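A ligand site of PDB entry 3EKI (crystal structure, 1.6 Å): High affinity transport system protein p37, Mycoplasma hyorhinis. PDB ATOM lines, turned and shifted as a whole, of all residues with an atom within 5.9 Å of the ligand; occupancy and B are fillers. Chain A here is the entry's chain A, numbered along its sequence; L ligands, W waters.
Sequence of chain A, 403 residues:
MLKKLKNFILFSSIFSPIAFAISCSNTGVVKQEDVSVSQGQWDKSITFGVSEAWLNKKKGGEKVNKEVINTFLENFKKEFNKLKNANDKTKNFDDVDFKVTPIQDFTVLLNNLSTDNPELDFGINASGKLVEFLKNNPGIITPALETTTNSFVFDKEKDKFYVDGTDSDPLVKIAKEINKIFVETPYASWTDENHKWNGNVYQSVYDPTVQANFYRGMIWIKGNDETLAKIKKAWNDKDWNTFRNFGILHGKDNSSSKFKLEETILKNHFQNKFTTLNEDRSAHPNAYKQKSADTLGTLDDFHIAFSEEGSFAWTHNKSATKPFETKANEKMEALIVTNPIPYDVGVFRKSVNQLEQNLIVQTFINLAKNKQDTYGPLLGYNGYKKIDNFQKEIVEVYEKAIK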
ATOM      1  N   ALA A 126      21.252 -24.495   4.456  1.00  0.00           N
ATOM      2  CA  ALA A 126      21.789 -25.167   3.266  1.00  0.00           C
ATOM      3  C   ALA A 126      20.777 -26.188   2.770  1.00  0.00           C
ATOM      4  O   ALA A 126      20.178 -26.903   3.591  1.00  0.00           O
ATOM      5  CB  ALA A 126      23.116 -25.803   3.616  1.00  0.00           C
ATOM      6  N   SER A 127      20.591 -26.265   1.463  1.00  0.00           N
ATOM      7  CA  SER A 127      19.570 -27.136   0.905  1.00  0.00           C
ATOM      8  C   SER A 127      19.783 -28.625   1.172  1.00  0.00           C
ATOM      9  O   SER A 127      18.885 -29.374   1.540  1.00  0.00           O
ATOM     10  CB  SER A 127      19.478 -26.889  -0.618  1.00  0.00           C
ATOM     11  OG  SER A 127      20.640 -27.349  -1.295  1.00  0.00           O
ATOM     12  N   LYS A 129      21.467 -30.251   3.542  1.00  0.00           N
ATOM     13  CA  LYS A 129      21.264 -30.561   4.948  1.00  0.00           C
ATOM     14  C   LYS A 129      19.770 -30.544   5.295  1.00  0.00           C
ATOM     15  O   LYS A 129      19.259 -31.330   6.080  1.00  0.00           O
ATOM     16  CB  LYS A 129      21.996 -29.567   5.827  1.00  0.00           C
ATOM     17  CG  LYS A 129      23.509 -29.753   5.819  1.00  0.00           C
ATOM     18  CD  LYS A 129      24.230 -28.571   6.425  1.00  0.00           C
ATOM     19  CE  LYS A 129      25.689 -28.945   6.703  1.00  0.00           C
ATOM     20  NZ  LYS A 129      26.590 -27.872   6.191  1.00  0.00           N
ATOM     21  N   THR A 149      22.098 -16.988  -6.256  1.00  0.00           N
ATOM     22  CA  THR A 149      23.357 -16.255  -6.120  1.00  0.00           C
ATOM     23  C   THR A 149      23.828 -15.770  -7.480  1.00  0.00           C
ATOM     24  O   THR A 149      23.493 -16.403  -8.489  1.00  0.00           O
ATOM     25  CB  THR A 149      24.369 -17.201  -5.424  1.00  0.00           C
ATOM     26  OG1 THR A 149      25.531 -16.485  -5.010  1.00  0.00           O
ATOM     27  CG2 THR A 149      24.855 -18.316  -6.338  1.00  0.00           C
ATOM     28  N   ASN A 200      33.413  -7.989   0.396  1.00  0.00           N
ATOM     29  CA  ASN A 200      32.627  -9.203   0.402  1.00  0.00           C
ATOM     30  C   ASN A 200      33.138 -10.295  -0.544  1.00  0.00           C
ATOM     31  O   ASN A 200      33.449 -11.413  -0.121  1.00  0.00           O
ATOM     32  CB  ASN A 200      31.184  -8.825   0.026  1.00  0.00           C
ATOM     33  CG  ASN A 200      30.224  -9.978   0.236  1.00  0.00           C
ATOM     34  OD1 ASN A 200      30.405 -10.749   1.183  1.00  0.00           O
ATOM     35  ND2 ASN A 200      29.228 -10.083  -0.625  1.00  0.00           N
ATOM     36  N   VAL A 201      33.192  -9.965  -1.823  1.00  0.00           N
ATOM     37  CA  VAL A 201      33.629 -10.824  -2.910  1.00  0.00           C
ATOM     38  C   VAL A 201      34.522 -10.052  -3.900  1.00  0.00           C
ATOM     39  O   VAL A 201      34.516  -8.829  -3.965  1.00  0.00           O
ATOM     40  CB  VAL A 201      32.468 -11.380  -3.767  1.00  0.00           C
ATOM     41  CG1 VAL A 201      31.474 -12.142  -2.894  1.00  0.00           C
ATOM     42  CG2 VAL A 201      31.790 -10.272  -4.523  1.00  0.00           C
ATOM     43  N   TYR A 206      32.267 -12.839 -11.182  1.00  0.00           N
ATOM     44  CA  TYR A 206      30.841 -13.073 -11.275  1.00  0.00           C
ATOM     45  C   TYR A 206      30.160 -12.361 -12.447  1.00  0.00           C
ATOM     46  O   TYR A 206      30.635 -11.325 -12.922  1.00  0.00           O
ATOM     47  CB  TYR A 206      30.153 -12.539 -10.015  1.00  0.00           C
ATOM     48  CG  TYR A 206      30.557 -13.179  -8.720  1.00  0.00           C
ATOM     49  CD1 TYR A 206      31.659 -12.784  -7.995  1.00  0.00           C
ATOM     50  CD2 TYR A 206      29.750 -14.198  -8.204  1.00  0.00           C
ATOM     51  CE1 TYR A 206      31.982 -13.398  -6.790  1.00  0.00           C
ATOM     52  CE2 TYR A 206      30.058 -14.829  -7.016  1.00  0.00           C
ATOM     53  CZ  TYR A 206      31.173 -14.418  -6.318  1.00  0.00           C
ATOM     54  OH  TYR A 206      31.479 -15.027  -5.126  1.00  0.00           O
ATOM     55  N   TYR A 215      24.651 -24.260  -6.638  1.00  0.00           N
ATOM     56  CA  TYR A 215      26.085 -24.143  -6.441  1.00  0.00           C
ATOM     57  C   TYR A 215      26.645 -25.564  -6.574  1.00  0.00           C
ATOM     58  O   TYR A 215      25.907 -26.564  -6.652  1.00  0.00           O
ATOM     59  CB  TYR A 215      26.511 -23.473  -5.132  1.00  0.00           C
ATOM     60  CG  TYR A 215      26.338 -24.322  -3.896  1.00  0.00           C
ATOM     61  CD1 TYR A 215      25.097 -24.852  -3.541  1.00  0.00           C
ATOM     62  CD2 TYR A 215      27.405 -24.599  -3.064  1.00  0.00           C
ATOM     63  CE1 TYR A 215      24.936 -25.623  -2.413  1.00  0.00           C
ATOM     64  CE2 TYR A 215      27.265 -25.377  -1.938  1.00  0.00           C
ATOM     65  CZ  TYR A 215      26.029 -25.888  -1.605  1.00  0.00           C
ATOM     66  OH  TYR A 215      25.893 -26.667  -0.492  1.00  0.00           O
ATOM     67  N   ASN A 254      28.678 -34.295   7.058  1.00  0.00           N
ATOM     68  CA  ASN A 254      27.321 -33.850   6.727  1.00  0.00           C
ATOM     69  C   ASN A 254      27.317 -32.663   5.776  1.00  0.00           C
ATOM     70  O   ASN A 254      26.254 -32.082   5.517  1.00  0.00           O
ATOM     71  CB  ASN A 254      26.542 -33.464   8.000  1.00  0.00           C
ATOM     72  CG  ASN A 254      27.181 -32.356   8.798  1.00  0.00           C
ATOM     73  OD1 ASN A 254      28.095 -31.655   8.381  1.00  0.00           O
ATOM     74  ND2 ASN A 254      26.699 -32.134  10.014  1.00  0.00           N
ATOM     75  N   SER A 255      28.511 -32.299   5.271  1.00  0.00           N
ATOM     76  CA  SER A 255      28.599 -31.227   4.297  1.00  0.00           C
ATOM     77  C   SER A 255      28.275 -31.691   2.876  1.00  0.00           C
ATOM     78  O   SER A 255      28.780 -32.710   2.413  1.00  0.00           O
ATOM     79  CB  SER A 255      30.007 -30.599   4.293  1.00  0.00           C
ATOM     80  OG  SER A 255      30.085 -29.620   3.253  1.00  0.00           O
ATOM     81  N   SER A 256      27.459 -30.959   2.122  1.00  0.00           N
ATOM     82  CA  SER A 256      27.277 -31.280   0.716  1.00  0.00           C
ATOM     83  C   SER A 256      28.529 -30.887  -0.078  1.00  0.00           C
ATOM     84  O   SER A 256      29.142 -31.755  -0.734  1.00  0.00           O
ATOM     85  CB  SER A 256      26.053 -30.599   0.101  1.00  0.00           C
ATOM     86  OG  SER A 256      24.867 -30.910   0.816  1.00  0.00           O
ATOM     87  N   SER A 257      28.918 -29.625  -0.049  1.00  0.00           N
ATOM     88  CA  SER A 257      29.966 -29.113  -0.910  1.00  0.00           C
ATOM     89  C   SER A 257      31.378 -29.373  -0.407  1.00  0.00           C
ATOM     90  O   SER A 257      32.318 -29.044  -1.161  1.00  0.00           O
ATOM     91  CB  SER A 257      29.810 -27.610  -1.149  1.00  0.00           C
ATOM     92  OG  SER A 257      29.971 -26.854   0.029  1.00  0.00           O
ATOM     93  N   LYS A 258      31.584 -29.885   0.784  1.00  0.00           N
ATOM     94  CA  LYS A 258      32.917 -30.214   1.295  1.00  0.00           C
ATOM     95  C   LYS A 258      33.037 -31.681   1.638  1.00  0.00           C
ATOM     96  O   LYS A 258      34.006 -32.140   2.264  1.00  0.00           O
ATOM     97  CB  LYS A 258      33.276 -29.302   2.473  1.00  0.00           C
ATOM     98  CG  LYS A 258      33.377 -27.847   2.022  1.00  0.00           C
ATOM     99  CD  LYS A 258      33.254 -26.880   3.189  1.00  0.00           C
ATOM    100  CE  LYS A 258      31.812 -26.731   3.610  1.00  0.00           C
ATOM    101  NZ  LYS A 258      31.142 -25.679   2.818  1.00  0.00           N
ATOM    102  N   GLU A 308      33.776 -25.627  -1.617  1.00  0.00           N
ATOM    103  CA  GLU A 308      32.781 -25.005  -2.466  1.00  0.00           C
ATOM    104  C   GLU A 308      33.426 -24.545  -3.762  1.00  0.00           C
ATOM    105  O   GLU A 308      34.539 -24.039  -3.722  1.00  0.00           O
ATOM    106  CB  GLU A 308      32.198 -23.777  -1.745  1.00  0.00           C
ATOM    107  CG  GLU A 308      31.722 -23.985  -0.327  1.00  0.00           C
ATOM    108  CD  GLU A 308      32.762 -23.733   0.728  1.00  0.00           C
ATOM    109  OE1 GLU A 308      32.350 -23.387   1.869  1.00  0.00           O
ATOM    110  OE2 GLU A 308      33.984 -23.880   0.447  1.00  0.00           O
ATOM    111  N   TRP A 314      35.220 -15.360  -2.428  1.00  0.00           N
ATOM    112  CA  TRP A 314      34.856 -14.608  -1.237  1.00  0.00           C
ATOM    113  C   TRP A 314      35.913 -14.677  -0.150  1.00  0.00           C
ATOM    114  O   TRP A 314      35.626 -14.446   1.044  1.00  0.00           O
ATOM    115  CB  TRP A 314      33.517 -15.113  -0.712  1.00  0.00           C
ATOM    116  CG  TRP A 314      33.376 -16.535  -0.326  1.00  0.00           C
ATOM    117  CD1 TRP A 314      33.757 -17.117   0.854  1.00  0.00           C
ATOM    118  CD2 TRP A 314      32.805 -17.582  -1.127  1.00  0.00           C
ATOM    119  NE1 TRP A 314      33.459 -18.462   0.820  1.00  0.00           N
ATOM    120  CE2 TRP A 314      32.874 -18.762  -0.380  1.00  0.00           C
ATOM    121  CE3 TRP A 314      32.243 -17.617  -2.401  1.00  0.00           C
ATOM    122  CZ2 TRP A 314      32.397 -19.992  -0.849  1.00  0.00           C
ATOM    123  CZ3 TRP A 314      31.777 -18.829  -2.861  1.00  0.00           C
ATOM    124  CH2 TRP A 314      31.852 -19.979  -2.101  1.00  0.00           C
ATOM    125  N   ILE A 341      23.586 -28.441  -6.842  1.00  0.00           N
ATOM    126  CA  ILE A 341      22.409 -28.563  -5.953  1.00  0.00           C
ATOM    127  C   ILE A 341      21.895 -27.174  -5.620  1.00  0.00           C
ATOM    128  O   ILE A 341      22.573 -26.181  -5.867  1.00  0.00           O
ATOM    129  CB  ILE A 341      22.746 -29.317  -4.663  1.00  0.00           C
ATOM    130  CG1 ILE A 341      23.770 -28.641  -3.761  1.00  0.00           C
ATOM    131  CG2 ILE A 341      23.165 -30.748  -5.010  1.00  0.00           C
ATOM    132  CD1 ILE A 341      23.964 -29.294  -2.402  1.00  0.00           C
ATOM    133  N   PRO A 342      20.677 -27.014  -5.111  1.00  0.00           N
ATOM    134  CA  PRO A 342      20.156 -25.658  -4.916  1.00  0.00           C
ATOM    135  C   PRO A 342      20.880 -24.837  -3.867  1.00  0.00           C
ATOM    136  O   PRO A 342      21.443 -25.378  -2.937  1.00  0.00           O
ATOM    137  CB  PRO A 342      18.717 -25.920  -4.437  1.00  0.00           C
ATOM    138  CG  PRO A 342      18.405 -27.280  -5.002  1.00  0.00           C
ATOM    139  CD  PRO A 342      19.697 -28.063  -4.748  1.00  0.00           C
ATOM    140  N   TYR A 343      20.834 -23.508  -4.042  1.00  0.00           N
ATOM    141  CA  TYR A 343      21.350 -22.629  -3.010  1.00  0.00           C
ATOM    142  C   TYR A 343      20.440 -22.728  -1.779  1.00  0.00           C
ATOM    143  O   TYR A 343      19.531 -23.553  -1.738  1.00  0.00           O
ATOM    144  CB  TYR A 343      21.479 -21.184  -3.511  1.00  0.00           C
ATOM    145  CG  TYR A 343      22.776 -20.512  -3.131  1.00  0.00           C
ATOM    146  CD1 TYR A 343      22.858 -19.388  -2.345  1.00  0.00           C
ATOM    147  CD2 TYR A 343      23.995 -21.041  -3.586  1.00  0.00           C
ATOM    148  CE1 TYR A 343      24.071 -18.805  -2.014  1.00  0.00           C
ATOM    149  CE2 TYR A 343      25.196 -20.465  -3.273  1.00  0.00           C
ATOM    150  CZ  TYR A 343      25.249 -19.331  -2.481  1.00  0.00           C
ATOM    151  OH  TYR A 343      26.462 -18.759  -2.163  1.00  0.00           O
ATOM    152  N   ASP A 344      20.682 -21.906  -0.771  1.00  0.00           N
ATOM    153  CA  ASP A 344      20.042 -22.083   0.533  1.00  0.00           C
ATOM    154  C   ASP A 344      18.528 -21.834   0.460  1.00  0.00           C
ATOM    155  O   ASP A 344      18.040 -21.117  -0.402  1.00  0.00           O
ATOM    156  CB  ASP A 344      20.690 -21.174   1.546  1.00  0.00           C
ATOM    157  CG  ASP A 344      22.095 -21.571   1.973  1.00  0.00           C
ATOM    158  OD1 ASP A 344      22.675 -22.449   1.287  1.00  0.00           O
ATOM    159  OD2 ASP A 344      22.585 -21.010   2.980  1.00  0.00           O
ATOM    160  N   PRO A 377      23.185 -10.376   0.446  1.00  0.00           N
ATOM    161  CA  PRO A 377      24.397 -10.424  -0.408  1.00  0.00           C
ATOM    162  C   PRO A 377      25.651 -10.701   0.392  1.00  0.00           C
ATOM    163  O   PRO A 377      26.644 -11.199  -0.178  1.00  0.00           O
ATOM    164  CB  PRO A 377      24.420  -9.063  -1.084  1.00  0.00           C
ATOM    165  CG  PRO A 377      22.983  -8.627  -1.031  1.00  0.00           C
ATOM    166  CD  PRO A 377      22.551  -9.051   0.341  1.00  0.00           C
ATOM    167  N   LEU A 378      25.666 -10.484   1.698  1.00  0.00           N
ATOM    168  CA  LEU A 378      26.838 -10.796   2.525  1.00  0.00           C
ATOM    169  C   LEU A 378      27.050 -12.307   2.698  1.00  0.00           C
ATOM    170  O   LEU A 378      28.115 -12.782   3.065  1.00  0.00           O
ATOM    171  CB  LEU A 378      26.749 -10.122   3.902  1.00  0.00           C
ATOM    172  CG  LEU A 378      26.796  -8.600   3.856  1.00  0.00           C
ATOM    173  CD1 LEU A 378      26.623  -8.024   5.250  1.00  0.00           C
ATOM    174  CD2 LEU A 378      28.108  -8.108   3.252  1.00  0.00           C
ATOM    175  N   LEU A 379      25.995 -13.047   2.419  1.00  0.00           N
ATOM    176  CA  LEU A 379      25.975 -14.493   2.509  1.00  0.00           C
ATOM    177  C   LEU A 379      25.966 -15.135   1.132  1.00  0.00           C
ATOM    178  O   LEU A 379      25.943 -16.363   1.005  1.00  0.00           O
ATOM    179  CB  LEU A 379      24.733 -14.953   3.298  1.00  0.00           C
ATOM    180  CG  LEU A 379      24.843 -14.932   4.820  1.00  0.00           C
ATOM    181  CD1 LEU A 379      25.059 -13.530   5.362  1.00  0.00           C
ATOM    182  CD2 LEU A 379      23.588 -15.549   5.431  1.00  0.00           C
ATOM    183  N   GLY A 380      25.930 -14.340   0.066  1.00  0.00           N
ATOM    184  CA  GLY A 380      25.830 -14.909  -1.262  1.00  0.00           C
ATOM    185  C   GLY A 380      24.421 -14.934  -1.801  1.00  0.00           C
ATOM    186  O   GLY A 380      24.136 -15.469  -2.866  1.00  0.00           O
ATOM    187  N   TYR A 381      23.451 -14.358  -1.070  1.00  0.00           N
ATOM    188  CA  TYR A 381      22.070 -14.381  -1.520  1.00  0.00           C
ATOM    189  C   TYR A 381      21.772 -13.104  -2.302  1.00  0.00           C
ATOM    190  O   TYR A 381      21.530 -12.054  -1.698  1.00  0.00           O
ATOM    191  CB  TYR A 381      21.079 -14.517  -0.366  1.00  0.00           C
ATOM    192  CG  TYR A 381      21.353 -15.593   0.631  1.00  0.00           C
ATOM    193  CD1 TYR A 381      21.995 -16.781   0.297  1.00  0.00           C
ATOM    194  CD2 TYR A 381      20.983 -15.447   1.981  1.00  0.00           C
ATOM    195  CE1 TYR A 381      22.257 -17.759   1.237  1.00  0.00           C
ATOM    196  CE2 TYR A 381      21.254 -16.438   2.903  1.00  0.00           C
ATOM    197  CZ  TYR A 381      21.888 -17.604   2.542  1.00  0.00           C
ATOM    198  OH  TYR A 381      22.128 -18.552   3.509  1.00  0.00           O
HETATM  199  N1  LIG L   1      29.339 -15.861  -1.145  1.00  0.00           N
HETATM  200  C1  LIG L   1      29.605 -15.057  -0.084  1.00  0.00           C
HETATM  201  C2  LIG L   1      29.683 -13.548  -0.297  1.00  0.00           C
HETATM  202  N2  LIG L   1      29.789 -15.583   1.140  1.00  0.00           N
HETATM  203  C3  LIG L   1      29.611 -16.922   1.330  1.00  0.00           C
HETATM  204  N3  LIG L   1      29.705 -17.407   2.562  1.00  0.00           N
HETATM  205  C4  LIG L   1      29.393 -17.775   0.236  1.00  0.00           C
HETATM  206  C5  LIG L   1      29.263 -17.183  -1.018  1.00  0.00           C
HETATM  207  C6  LIG L   1      29.258 -19.298   0.317  1.00  0.00           C
HETATM  208  N4  LIG L   1      27.908 -19.826   0.547  1.00  0.00           N
HETATM  209  C7  LIG L   1      26.959 -19.194   1.240  1.00  0.00           C
HETATM  210  S1  LIG L   1      25.504 -20.165   1.239  1.00  0.00           S
HETATM  211  C8  LIG L   1      26.263 -21.434   0.304  1.00  0.00           C
HETATM  212  C9  LIG L   1      27.593 -21.088   0.147  1.00  0.00           C
HETATM  213  C10 LIG L   1      28.515 -21.863  -0.818  1.00  0.00           C
HETATM  214  C11 LIG L   1      25.595 -22.757  -0.066  1.00  0.00           C
HETATM  215  C12 LIG L   1      25.527 -23.683   1.147  1.00  0.00           C
HETATM  216  O1  LIG L   1      26.872 -24.029   1.546  1.00  0.00           O
HETATM  217  P1  LIG L   1      27.301 -24.516   3.001  1.00  0.00           P
HETATM  218  O2  LIG L   1      28.773 -24.444   3.102  1.00  0.00           O
HETATM  219  O3  LIG L   1      26.563 -23.737   4.052  1.00  0.00           O
HETATM  220  O4  LIG L   1      26.750 -25.984   3.185  1.00  0.00           O
HETATM  221  P2  LIG L   1      27.492 -27.344   2.771  1.00  0.00           P
HETATM  222  O5  LIG L   1      27.684 -27.380   1.281  1.00  0.00           O
HETATM  223  O6  LIG L   1      26.501 -28.471   3.264  1.00  0.00           O
HETATM  224  O7  LIG L   1      28.829 -27.500   3.603  1.00  0.00           O
HETATM  225  O   HOH W   1      29.288 -26.685   6.003  1.00  0.00           O
HETATM  226  O   HOH W   2      24.486 -21.816   4.519  1.00  0.00           O
HETATM  227  O   HOH W   3      29.102 -15.406  -3.826  1.00  0.00           O
HETATM  228  O   HOH W   4      25.546 -25.247   6.338  1.00  0.00           O
HETATM  229  O   HOH W   5      24.093 -28.919   2.399  1.00  0.00           O
HETATM  230  O   HOH W   6      29.414 -20.008   3.857  1.00  0.00           O
HETATM  231  O   HOH W   7      30.092 -22.040   2.318  1.00  0.00           O
HETATM  232  O   HOH W   8      31.712 -14.499   3.346  1.00  0.00           O
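The side-chain hydroxyl of Ser 255 lies within hydrogen-bond range of an oxygen (O7) of the ligand, 2.5 Å away.
OH of Tyr 215 lies within hydrogen-bond range of O5 of the ligand.
An oxygen (O5) of the ligand is in hydrogen-bond range of the backbone NH of Ser 257 (2.9 Å).
The side-chain hydroxyl of Ser 257 is in hydrogen-bond range of an oxygen (O5) of the ligand (2.7 Å).
O2 of the ligand is in salt-bridge range of NZ of Lys 258, at 2.7 Å.
The backbone NH of Ser 256 sits at hydrogen-bond distance from an oxygen (O6) of the ligand (2.9 Å).
O6 of the ligand lies within salt-bridge range of NZ of Lys 129, 3.0 Å away.
OG of Ser 255 sits at hydrogen-bond distance from N of Lys 258, at 2.9 Å.
N of Tyr 215 sits at hydrogen-bond distance from O of Ile 341 (2.9 Å).
OG of Ser 257 lies within hydrogen-bond range of NZ of Lys 258 (3.2 Å).
NZ of Lys 258 lies within salt-bridge range of OE1 of Glu 308 (2.8 Å).
The side-chain carboxylate of Asp 344 sits at hydrogen-bond distance from the side-chain hydroxyl of Tyr 381, 2.6 Å away.
ND2 of Asn 200 lies within hydrogen-bond range of O of Pro 377, at 2.8 Å.
The backbone carbonyl oxygen (O) of Gly 380 lies within hydrogen-bond range of the side-chain hydroxyl (OG1) of Thr 149, 2.8 Å away.
A nitrogen (N4) of the ligand sits close to the side-chain hydroxyl of Tyr 343, at 3.3 Å.
The side-chain carboxylate (OD2) of Asp 344 lies close to a sulfur (S1) of the ligand, at 3.5 Å.
Merely in contact with the ligand: Ala 126 (3.7 Å), Asn 200 (3.2 Å), Val 201 (3.5 Å), Glu 308 (3.9 Å), Trp 314 (3.3 Å), Pro 377 (3.8 Å), Leu 378 (3.8 Å), Leu 379 (3.0 Å) and Gly 380 (3.6 Å).
Hydrophobic or aromatic side chains that line the ligand: Ala 126, Val 201, Tyr 215, Trp 314 and Tyr 343.
Within 4 Å of the ligand: Ala 126, Lys 129, Asn 200, Val 201, Tyr 215, Ser 255, Ser 256, Ser 257, Lys 258, Glu 308, Trp 314, Tyr 343, Asp 344, Pro 377, Leu 378, Leu 379 and Gly 380.
The nearest printed residue that does not touch the ligand is Tyr 381 (4.04 Å).
Water W1 lies within hydrogen-bond range of an oxygen (O7) of the ligand (2.6 Å) and the side-chain amino group of Lys 129 (3.0 Å).
Water W5 lies within hydrogen-bond range of O6 of the ligand (2.6 Å), OG of Ser 256 (2.7 Å) and N of Lys 129 (3.2 Å).
Water W3 bridges N1 of the ligand and OH of Tyr 206.
Water W7 bridges OE1 of Glu 308 and O2 of the ligand.
Water W2 lies within hydrogen-bond range of the side-chain carboxylate (OD2) of Asp 344 (2.6 Å) and an oxygen (O3) of the ligand (2.9 Å).
Water W4 bridges the side-chain amino group of Lys 129 and an oxygen (O3) of the ligand.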
